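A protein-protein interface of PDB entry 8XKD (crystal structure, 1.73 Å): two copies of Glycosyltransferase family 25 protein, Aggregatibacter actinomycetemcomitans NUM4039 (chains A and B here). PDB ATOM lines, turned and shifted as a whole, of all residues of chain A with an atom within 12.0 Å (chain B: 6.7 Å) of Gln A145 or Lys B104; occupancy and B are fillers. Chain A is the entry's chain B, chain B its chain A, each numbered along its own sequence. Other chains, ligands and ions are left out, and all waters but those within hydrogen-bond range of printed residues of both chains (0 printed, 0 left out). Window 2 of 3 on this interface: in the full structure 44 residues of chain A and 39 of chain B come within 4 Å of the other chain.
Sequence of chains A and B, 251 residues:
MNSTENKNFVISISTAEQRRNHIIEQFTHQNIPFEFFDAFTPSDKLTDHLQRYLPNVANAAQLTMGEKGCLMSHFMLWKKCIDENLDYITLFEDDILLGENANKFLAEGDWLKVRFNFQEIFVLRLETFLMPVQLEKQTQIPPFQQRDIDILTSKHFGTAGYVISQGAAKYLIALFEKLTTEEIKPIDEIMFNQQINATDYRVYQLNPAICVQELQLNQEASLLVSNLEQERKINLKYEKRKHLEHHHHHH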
ATOM      1  N   LYS A 137      24.880   8.305  -4.662  1.00  0.00           N
ATOM      2  CA  LYS A 137      25.086   8.364  -3.222  1.00  0.00           C
ATOM      3  C   LYS A 137      26.403   7.688  -2.892  1.00  0.00           C
ATOM      4  O   LYS A 137      26.908   6.849  -3.655  1.00  0.00           O
ATOM      5  CB  LYS A 137      23.950   7.661  -2.454  1.00  0.00           C
ATOM      6  CG  LYS A 137      22.563   8.223  -2.687  1.00  0.00           C
ATOM      7  CD  LYS A 137      22.373   9.570  -2.016  1.00  0.00           C
ATOM      8  CE  LYS A 137      21.467  10.480  -2.843  1.00  0.00           C
ATOM      9  NZ  LYS A 137      21.424  11.884  -2.323  1.00  0.00           N
ATOM     10  N   GLN A 138      26.982   8.075  -1.765  1.00  0.00           N
ATOM     11  CA  GLN A 138      28.161   7.401  -1.246  1.00  0.00           C
ATOM     12  C   GLN A 138      28.111   7.360   0.281  1.00  0.00           C
ATOM     13  O   GLN A 138      27.324   8.057   0.904  1.00  0.00           O
ATOM     14  CB  GLN A 138      29.448   8.053  -1.757  1.00  0.00           C
ATOM     15  CG  GLN A 138      29.559   9.552  -1.531  1.00  0.00           C
ATOM     16  CD  GLN A 138      29.872   9.900  -0.100  1.00  0.00           C
ATOM     17  OE1 GLN A 138      30.819   9.381   0.481  1.00  0.00           O
ATOM     18  NE2 GLN A 138      29.079  10.791   0.479  1.00  0.00           N
ATOM     19  N   ILE A 141      31.657   9.695   3.128  1.00  0.00           N
ATOM     20  CA  ILE A 141      31.610  11.097   3.582  1.00  0.00           C
ATOM     21  C   ILE A 141      30.234  11.406   4.176  1.00  0.00           C
ATOM     22  O   ILE A 141      29.228  11.365   3.475  1.00  0.00           O
ATOM     23  CB  ILE A 141      31.930  12.042   2.406  1.00  0.00           C
ATOM     24  CG1 ILE A 141      33.290  11.678   1.801  1.00  0.00           C
ATOM     25  CG2 ILE A 141      31.893  13.498   2.865  1.00  0.00           C
ATOM     26  CD1 ILE A 141      33.587  12.332   0.454  1.00  0.00           C
ATOM     27  N   PRO A 142      30.169  11.706   5.487  1.00  0.00           N
ATOM     28  CA  PRO A 142      28.848  11.842   6.100  1.00  0.00           C
ATOM     29  C   PRO A 142      28.093  13.088   5.633  1.00  0.00           C
ATOM     30  O   PRO A 142      28.722  14.065   5.241  1.00  0.00           O
ATOM     31  CB  PRO A 142      29.166  11.977   7.584  1.00  0.00           C
ATOM     32  CG  PRO A 142      30.550  12.524   7.614  1.00  0.00           C
ATOM     33  CD  PRO A 142      31.245  11.865   6.473  1.00  0.00           C
ATOM     34  N   PRO A 143      26.762  13.039   5.679  1.00  0.00           N
ATOM     35  CA  PRO A 143      25.979  14.185   5.241  1.00  0.00           C
ATOM     36  C   PRO A 143      26.138  15.300   6.251  1.00  0.00           C
ATOM     37  O   PRO A 143      26.719  15.092   7.329  1.00  0.00           O
ATOM     38  CB  PRO A 143      24.548  13.657   5.213  1.00  0.00           C
ATOM     39  CG  PRO A 143      24.565  12.542   6.223  1.00  0.00           C
ATOM     40  CD  PRO A 143      25.904  11.902   6.051  1.00  0.00           C
ATOM     41  N   PHE A 144      25.699  16.489   5.862  1.00  0.00           N
ATOM     42  CA  PHE A 144      25.783  17.649   6.720  1.00  0.00           C
ATOM     43  C   PHE A 144      24.495  18.445   6.615  1.00  0.00           C
ATOM     44  O   PHE A 144      24.060  18.806   5.502  1.00  0.00           O
ATOM     45  CB  PHE A 144      26.972  18.526   6.319  1.00  0.00           C
ATOM     46  CG  PHE A 144      27.181  19.717   7.225  1.00  0.00           C
ATOM     47  CD1 PHE A 144      27.376  19.539   8.590  1.00  0.00           C
ATOM     48  CD2 PHE A 144      27.195  21.004   6.720  1.00  0.00           C
ATOM     49  CE1 PHE A 144      27.594  20.620   9.433  1.00  0.00           C
ATOM     50  CE2 PHE A 144      27.376  22.088   7.551  1.00  0.00           C
ATOM     51  CZ  PHE A 144      27.590  21.909   8.904  1.00  0.00           C
ATOM     52  N   GLN A 145      23.889  18.733   7.772  1.00  0.00           N
ATOM     53  CA  GLN A 145      22.658  19.526   7.829  1.00  0.00           C
ATOM     54  C   GLN A 145      21.588  19.001   6.857  1.00  0.00           C
ATOM     55  O   GLN A 145      20.959  19.769   6.132  1.00  0.00           O
ATOM     56  CB  GLN A 145      22.979  21.004   7.547  1.00  0.00           C
ATOM     57  CG  GLN A 145      23.893  21.617   8.592  1.00  0.00           C
ATOM     58  CD  GLN A 145      23.207  21.740   9.935  1.00  0.00           C
ATOM     59  OE1 GLN A 145      23.612  21.124  10.923  1.00  0.00           O
ATOM     60  NE2 GLN A 145      22.136  22.513   9.972  1.00  0.00           N
ATOM     61  N   GLN A 146      21.431  17.685   6.857  1.00  0.00           N
ATOM     62  CA  GLN A 146      20.465  16.951   6.016  1.00  0.00           C
ATOM     63  C   GLN A 146      20.719  17.049   4.517  1.00  0.00           C
ATOM     64  O   GLN A 146      19.815  16.855   3.719  1.00  0.00           O
ATOM     65  CB  GLN A 146      19.013  17.337   6.334  1.00  0.00           C
ATOM     66  CG  GLN A 146      18.545  16.947   7.722  1.00  0.00           C
ATOM     67  CD  GLN A 146      17.115  17.400   7.980  1.00  0.00           C
ATOM     68  OE1 GLN A 146      16.440  17.940   7.088  1.00  0.00           O
ATOM     69  NE2 GLN A 146      16.639  17.177   9.206  1.00  0.00           N
ATOM     70  N   ARG A 147      21.948  17.363   4.132  1.00  0.00           N
ATOM     71  CA  ARG A 147      22.313  17.348   2.736  1.00  0.00           C
ATOM     72  C   ARG A 147      23.372  16.288   2.517  1.00  0.00           C
ATOM     73  O   ARG A 147      24.353  16.191   3.256  1.00  0.00           O
ATOM     74  CB  ARG A 147      22.761  18.739   2.288  1.00  0.00           C
ATOM     75  CG  ARG A 147      21.587  19.702   2.358  1.00  0.00           C
ATOM     76  CD  ARG A 147      21.945  21.139   2.100  1.00  0.00           C
ATOM     77  NE  ARG A 147      21.006  22.009   2.805  1.00  0.00           N
ATOM     78  CZ  ARG A 147      20.015  22.663   2.221  1.00  0.00           C
ATOM     79  NH1 ARG A 147      19.209  23.428   2.950  1.00  0.00           N
ATOM     80  NH2 ARG A 147      19.839  22.564   0.914  1.00  0.00           N
ATOM     81  N   ASP A 148      23.150  15.472   1.511  1.00  0.00           N
ATOM     82  CA  ASP A 148      24.103  14.461   1.152  1.00  0.00           C
ATOM     83  C   ASP A 148      25.199  15.087   0.298  1.00  0.00           C
ATOM     84  O   ASP A 148      24.972  16.081  -0.412  1.00  0.00           O
ATOM     85  CB  ASP A 148      23.429  13.359   0.333  1.00  0.00           C
ATOM     86  CG  ASP A 148      22.484  12.505   1.156  1.00  0.00           C
ATOM     87  OD1 ASP A 148      22.732  12.354   2.366  1.00  0.00           O
ATOM     88  OD2 ASP A 148      21.493  12.010   0.577  1.00  0.00           O
ATOM     89  N   ILE A 149      26.360  14.464   0.350  1.00  0.00           N
ATOM     90  CA  ILE A 149      27.420  14.741  -0.565  1.00  0.00           C
ATOM     91  C   ILE A 149      27.393  13.597  -1.578  1.00  0.00           C
ATOM     92  O   ILE A 149      27.816  12.475  -1.281  1.00  0.00           O
ATOM     93  CB  ILE A 149      28.771  14.797   0.162  1.00  0.00           C
ATOM     94  CG1 ILE A 149      28.792  15.847   1.259  1.00  0.00           C
ATOM     95  CG2 ILE A 149      29.912  15.011  -0.828  1.00  0.00           C
ATOM     96  CD1 ILE A 149      28.371  17.201   0.807  1.00  0.00           C
ATOM     97  N   ASP A 150      26.844  13.872  -2.758  1.00  0.00           N
ATOM     98  CA  ASP A 150      26.815  12.885  -3.843  1.00  0.00           C
ATOM     99  C   ASP A 150      28.010  13.043  -4.765  1.00  0.00           C
ATOM    100  O   ASP A 150      28.675  14.083  -4.779  1.00  0.00           O
ATOM    101  CB  ASP A 150      25.544  13.035  -4.648  1.00  0.00           C
ATOM    102  CG  ASP A 150      24.305  12.641  -3.871  1.00  0.00           C
ATOM    103  OD1 ASP A 150      24.417  12.065  -2.777  1.00  0.00           O
ATOM    104  OD2 ASP A 150      23.216  12.898  -4.400  1.00  0.00           O
ATOM    105  N   GLN B  30      22.296  36.612   5.970  1.00  0.00           N
ATOM    106  CA  GLN B  30      22.693  35.338   6.563  1.00  0.00           C
ATOM    107  C   GLN B  30      24.039  35.365   7.242  1.00  0.00           C
ATOM    108  O   GLN B  30      24.530  34.291   7.634  1.00  0.00           O
ATOM    109  CB  GLN B  30      22.603  34.223   5.512  1.00  0.00           C
ATOM    110  CG  GLN B  30      21.207  33.931   5.007  1.00  0.00           C
ATOM    111  CD  GLN B  30      21.096  32.600   4.250  1.00  0.00           C
ATOM    112  OE1 GLN B  30      21.512  31.563   4.743  1.00  0.00           O
ATOM    113  NE2 GLN B  30      20.472  32.621   3.087  1.00  0.00           N
ATOM    114  N   ILE B  32      27.040  35.814   6.133  1.00  0.00           N
ATOM    115  CA  ILE B  32      28.056  35.054   5.407  1.00  0.00           C
ATOM    116  C   ILE B  32      29.098  36.028   4.880  1.00  0.00           C
ATOM    117  O   ILE B  32      28.760  36.891   4.069  1.00  0.00           O
ATOM    118  CB  ILE B  32      27.440  34.286   4.221  1.00  0.00           C
ATOM    119  CG1 ILE B  32      26.325  33.359   4.679  1.00  0.00           C
ATOM    120  CG2 ILE B  32      28.535  33.553   3.476  1.00  0.00           C
ATOM    121  CD1 ILE B  32      25.445  32.875   3.545  1.00  0.00           C
ATOM    122  N   ASN B 101      19.290  28.057   4.505  1.00  0.00           N
ATOM    123  CA  ASN B 101      20.228  27.727   5.585  1.00  0.00           C
ATOM    124  C   ASN B 101      21.682  27.743   5.105  1.00  0.00           C
ATOM    125  O   ASN B 101      22.529  26.938   5.528  1.00  0.00           O
ATOM    126  CB  ASN B 101      19.805  26.396   6.205  1.00  0.00           C
ATOM    127  CG  ASN B 101      18.465  26.501   6.928  1.00  0.00           C
ATOM    128  OD1 ASN B 101      17.498  25.821   6.578  1.00  0.00           O
ATOM    129  ND2 ASN B 101      18.396  27.389   7.925  1.00  0.00           N
ATOM    130  N   ALA B 102      21.966  28.694   4.210  1.00  0.00           N
ATOM    131  CA  ALA B 102      23.276  28.724   3.548  1.00  0.00           C
ATOM    132  C   ALA B 102      24.432  29.022   4.517  1.00  0.00           C
ATOM    133  O   ALA B 102      25.533  28.567   4.298  1.00  0.00           O
ATOM    134  CB  ALA B 102      23.242  29.720   2.384  1.00  0.00           C
ATOM    135  N   ASN B 103      24.149  29.801   5.575  1.00  0.00           N
ATOM    136  CA  ASN B 103      25.108  30.169   6.605  1.00  0.00           C
ATOM    137  C   ASN B 103      25.866  28.970   7.179  1.00  0.00           C
ATOM    138  O   ASN B 103      27.066  29.034   7.380  1.00  0.00           O
ATOM    139  CB  ASN B 103      24.354  30.890   7.726  1.00  0.00           C
ATOM    140  CG  ASN B 103      23.057  30.197   8.061  1.00  0.00           C
ATOM    141  OD1 ASN B 103      23.059  29.169   8.731  1.00  0.00           O
ATOM    142  ND2 ASN B 103      21.936  30.738   7.572  1.00  0.00           N
ATOM    143  N   LYS B 104      25.161  27.862   7.406  1.00  0.00           N
ATOM    144  CA  LYS B 104      25.795  26.701   8.024  1.00  0.00           C
ATOM    145  C   LYS B 104      26.888  26.134   7.139  1.00  0.00           C
ATOM    146  O   LYS B 104      27.867  25.563   7.630  1.00  0.00           O
ATOM    147  CB  LYS B 104      24.753  25.617   8.292  1.00  0.00           C
ATOM    148  CG  LYS B 104      23.654  25.993   9.289  1.00  0.00           C
ATOM    149  CD  LYS B 104      24.203  26.361  10.663  1.00  0.00           C
ATOM    150  CE  LYS B 104      24.375  25.155  11.584  1.00  0.00           C
ATOM    151  NZ  LYS B 104      24.522  25.604  13.003  1.00  0.00           N
ATOM    152  N   PHE B 105      26.723  26.310   5.822  1.00  0.00           N
ATOM    153  CA  PHE B 105      27.686  25.812   4.843  1.00  0.00           C
ATOM    154  C   PHE B 105      28.765  26.822   4.491  1.00  0.00           C
ATOM    155  O   PHE B 105      29.887  26.463   4.230  1.00  0.00           O
ATOM    156  CB  PHE B 105      26.935  25.395   3.573  1.00  0.00           C
ATOM    157  CG  PHE B 105      25.960  24.294   3.804  1.00  0.00           C
ATOM    158  CD1 PHE B 105      24.688  24.572   4.293  1.00  0.00           C
ATOM    159  CD2 PHE B 105      26.318  22.974   3.573  1.00  0.00           C
ATOM    160  CE1 PHE B 105      23.784  23.561   4.551  1.00  0.00           C
ATOM    161  CE2 PHE B 105      25.398  21.970   3.791  1.00  0.00           C
ATOM    162  CZ  PHE B 105      24.151  22.262   4.295  1.00  0.00           C
ATOM    163  N   LEU B 106      28.425  28.101   4.482  1.00  0.00           N
ATOM    164  CA  LEU B 106      29.275  29.110   3.864  1.00  0.00           C
ATOM    165  C   LEU B 106      29.963  30.035   4.846  1.00  0.00           C
ATOM    166  O   LEU B 106      30.926  30.688   4.500  1.00  0.00           O
ATOM    167  CB  LEU B 106      28.433  29.972   2.901  1.00  0.00           C
ATOM    168  CG  LEU B 106      27.807  29.173   1.777  1.00  0.00           C
ATOM    169  CD1 LEU B 106      27.005  30.120   0.870  1.00  0.00           C
ATOM    170  CD2 LEU B 106      28.888  28.419   0.993  1.00  0.00           C
ATOM    171  N   ALA B 107      29.471  30.094   6.076  1.00  0.00           N
ATOM    172  CA  ALA B 107      30.066  30.967   7.087  1.00  0.00           C
ATOM    173  C   ALA B 107      31.048  30.201   7.974  1.00  0.00           C
ATOM    174  O   ALA B 107      31.705  30.790   8.837  1.00  0.00           O
ATOM    175  CB  ALA B 107      28.954  31.555   7.921  1.00  0.00           C
ATOM    176  N   GLU B 108      31.144  28.899   7.753  1.00  0.00           N
ATOM    177  CA  GLU B 108      32.019  28.030   8.545  1.00  0.00           C
ATOM    178  C   GLU B 108      32.505  26.928   7.630  1.00  0.00           C
ATOM    179  O   GLU B 108      31.750  26.451   6.808  1.00  0.00           O
ATOM    180  CB  GLU B 108      31.239  27.449   9.735  1.00  0.00           C
ATOM    181  CG  GLU B 108      31.926  26.327  10.488  1.00  0.00           C
ATOM    182  CD  GLU B 108      33.187  26.756  11.222  1.00  0.00           C
ATOM    183  OE1 GLU B 108      33.097  27.647  12.103  1.00  0.00           O
ATOM    184  OE2 GLU B 108      34.259  26.186  10.942  1.00  0.00           O
ATOM    185  N   GLY B 109      33.766  26.539   7.774  1.00  0.00           N
ATOM    186  CA  GLY B 109      34.358  25.513   6.941  1.00  0.00           C
ATOM    187  C   GLY B 109      34.800  24.254   7.663  1.00  0.00           C
ATOM    188  O   GLY B 109      35.314  23.345   7.031  1.00  0.00           O
ATOM    189  N   ASP B 110      34.544  24.155   8.964  1.00  0.00           N
ATOM    190  CA  ASP B 110      35.029  22.959   9.688  1.00  0.00           C
ATOM    191  C   ASP B 110      34.339  21.678   9.162  1.00  0.00           C
ATOM    192  O   ASP B 110      34.967  20.625   9.121  1.00  0.00           O
ATOM    193  CB  ASP B 110      35.025  23.115  11.214  1.00  0.00           C
ATOM    194  CG  ASP B 110      33.677  23.332  11.796  1.00  0.00           C
ATOM    195  OD1 ASP B 110      32.642  23.129  11.097  1.00  0.00           O
ATOM    196  OD2 ASP B 110      33.656  23.696  13.003  1.00  0.00           O
ATOM    197  N   TRP B 111      33.104  21.794   8.680  1.00  0.00           N
ATOM    198  CA  TRP B 111      32.394  20.671   8.070  1.00  0.00           C
ATOM    199  C   TRP B 111      33.098  20.128   6.834  1.00  0.00           C
ATOM    200  O   TRP B 111      33.034  18.930   6.560  1.00  0.00           O
ATOM    201  CB  TRP B 111      30.942  21.003   7.767  1.00  0.00           C
ATOM    202  CG  TRP B 111      30.776  22.031   6.693  1.00  0.00           C
ATOM    203  CD1 TRP B 111      30.865  23.379   6.832  1.00  0.00           C
ATOM    204  CD2 TRP B 111      30.470  21.785   5.324  1.00  0.00           C
ATOM    205  NE1 TRP B 111      30.654  24.001   5.622  1.00  0.00           N
ATOM    206  CE2 TRP B 111      30.396  23.045   4.681  1.00  0.00           C
ATOM    207  CE3 TRP B 111      30.241  20.633   4.579  1.00  0.00           C
ATOM    208  CZ2 TRP B 111      30.125  23.173   3.316  1.00  0.00           C
ATOM    209  CZ3 TRP B 111      29.951  20.764   3.216  1.00  0.00           C
ATOM    210  CH2 TRP B 111      29.881  22.028   2.608  1.00  0.00           C
ATOM    211  N   ARG B 115      35.364  16.389   6.276  1.00  0.00           N
ATOM    212  CA  ARG B 115      34.884  15.536   5.208  1.00  0.00           C
ATOM    213  C   ARG B 115      35.870  15.335   4.066  1.00  0.00           C
ATOM    214  O   ARG B 115      35.741  14.355   3.353  1.00  0.00           O
ATOM    215  CB  ARG B 115      33.574  16.087   4.673  1.00  0.00           C
ATOM    216  CG  ARG B 115      32.420  15.779   5.594  1.00  0.00           C
ATOM    217  CD  ARG B 115      31.138  16.549   5.272  1.00  0.00           C
ATOM    218  NE  ARG B 115      30.087  16.246   6.232  1.00  0.00           N
ATOM    219  CZ  ARG B 115      30.097  16.642   7.507  1.00  0.00           C
ATOM    220  NH1 ARG B 115      31.077  17.413   7.993  1.00  0.00           N
ATOM    221  NH2 ARG B 115      29.124  16.281   8.313  1.00  0.00           N
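The guanidinium group (NE) of Arg B115 sits at hydrogen-bond distance from the backbone carbonyl oxygen (O) of Pro A142 (2.8 Å). The guanidinium group (NH2) of Arg B115 lies within hydrogen-bond range of the backbone carbonyl oxygen (O) of Pro A143 (2.9 Å).
The side-chain amide oxygen (OE1) of Gln A138 sits at hydrogen-bond distance from the backbone NH (N) of Ile A141 (2.8 Å). The backbone carbonyl oxygen of Trp B111 sits at hydrogen-bond distance from the guanidinium group of Arg B115, at 2.9 Å. The backbone carbonyl oxygen (O) of Glu B108 lies within hydrogen-bond range of the indole nitrogen (NE1) of Trp B111 (2.9 Å). The backbone carbonyl oxygen (O) of Phe B105 sits at hydrogen-bond distance from the indole nitrogen (NE1) of Trp B111 (2.9 Å).
Ile A141 touches Arg B115 (CG2 to CB, 3.6 Å). O of Lys B104 touches CE2 of Phe A144, 3.5 Å away. Phe A144 touches Phe B105. CE2 of Phe A144 touches CG of Trp B111, 3.5 Å away. Phe A144 touches Arg B115. Lys B104 touches Gln A145. Phe B105 touches Gln A145 (CZ to CB, 3.7 Å). Arg A147 touches Phe B105 (CD to CZ, 3.3 Å).
Lys B104 touches just these residues of chain A: Phe A144 and Gln A145. No residue of chain A comes within 4 Å of Ala B102. No residue of chain A comes within 4 Å of Gly B109. Printed residues of chain B within 4 Å of Phe A144: Lys B104 (3.5 Å), Phe B105 (3.6 Å), Trp B111 (3.5 Å) and Arg B115 (3.7 Å). Of the printed residues of chain B, Ile A141 touches Arg B115 (3.6 Å). Of the printed residues of chain B, Arg A147 touches Phe B105. Printed residues of chain A within 4 Å of Phe B105: Phe A144 (3.6 Å), Gln A145 (3.7 Å) and Arg A147 (3.3 Å). Gln A146 touches none of the printed residues of chain B. Asp A150 touches none of the printed residues of chain B. The nearest printed residue of chain A that does not touch Lys B104 is Arg A147 (7.6 Å). The nearest printed residue of chain B that does not touch Pro A143 is Trp B111 (6.9 Å).
Hydrophobic or aromatic side chains of chain A that line the printed part of chain B: Ile A141, Pro A142 and Phe A144. Of the 14 printed residues of chain B, 4 touch a printed residue of chain A. Printed residues of chain B that touch a printed residue of chain A: Lys B104, Phe B105, Trp B111 and Arg B115. Hydrophobic or aromatic side chains of chain B that line the printed part of chain A: Phe B105 and Trp B111. Among the printed residues, 10 pairs touch across the chains. Among the printed residues, no Asp or Glu carboxylate lies within 4 Å of a Lys or Arg side-chain nitrogen of the other chain.
No position is printed for both chains.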
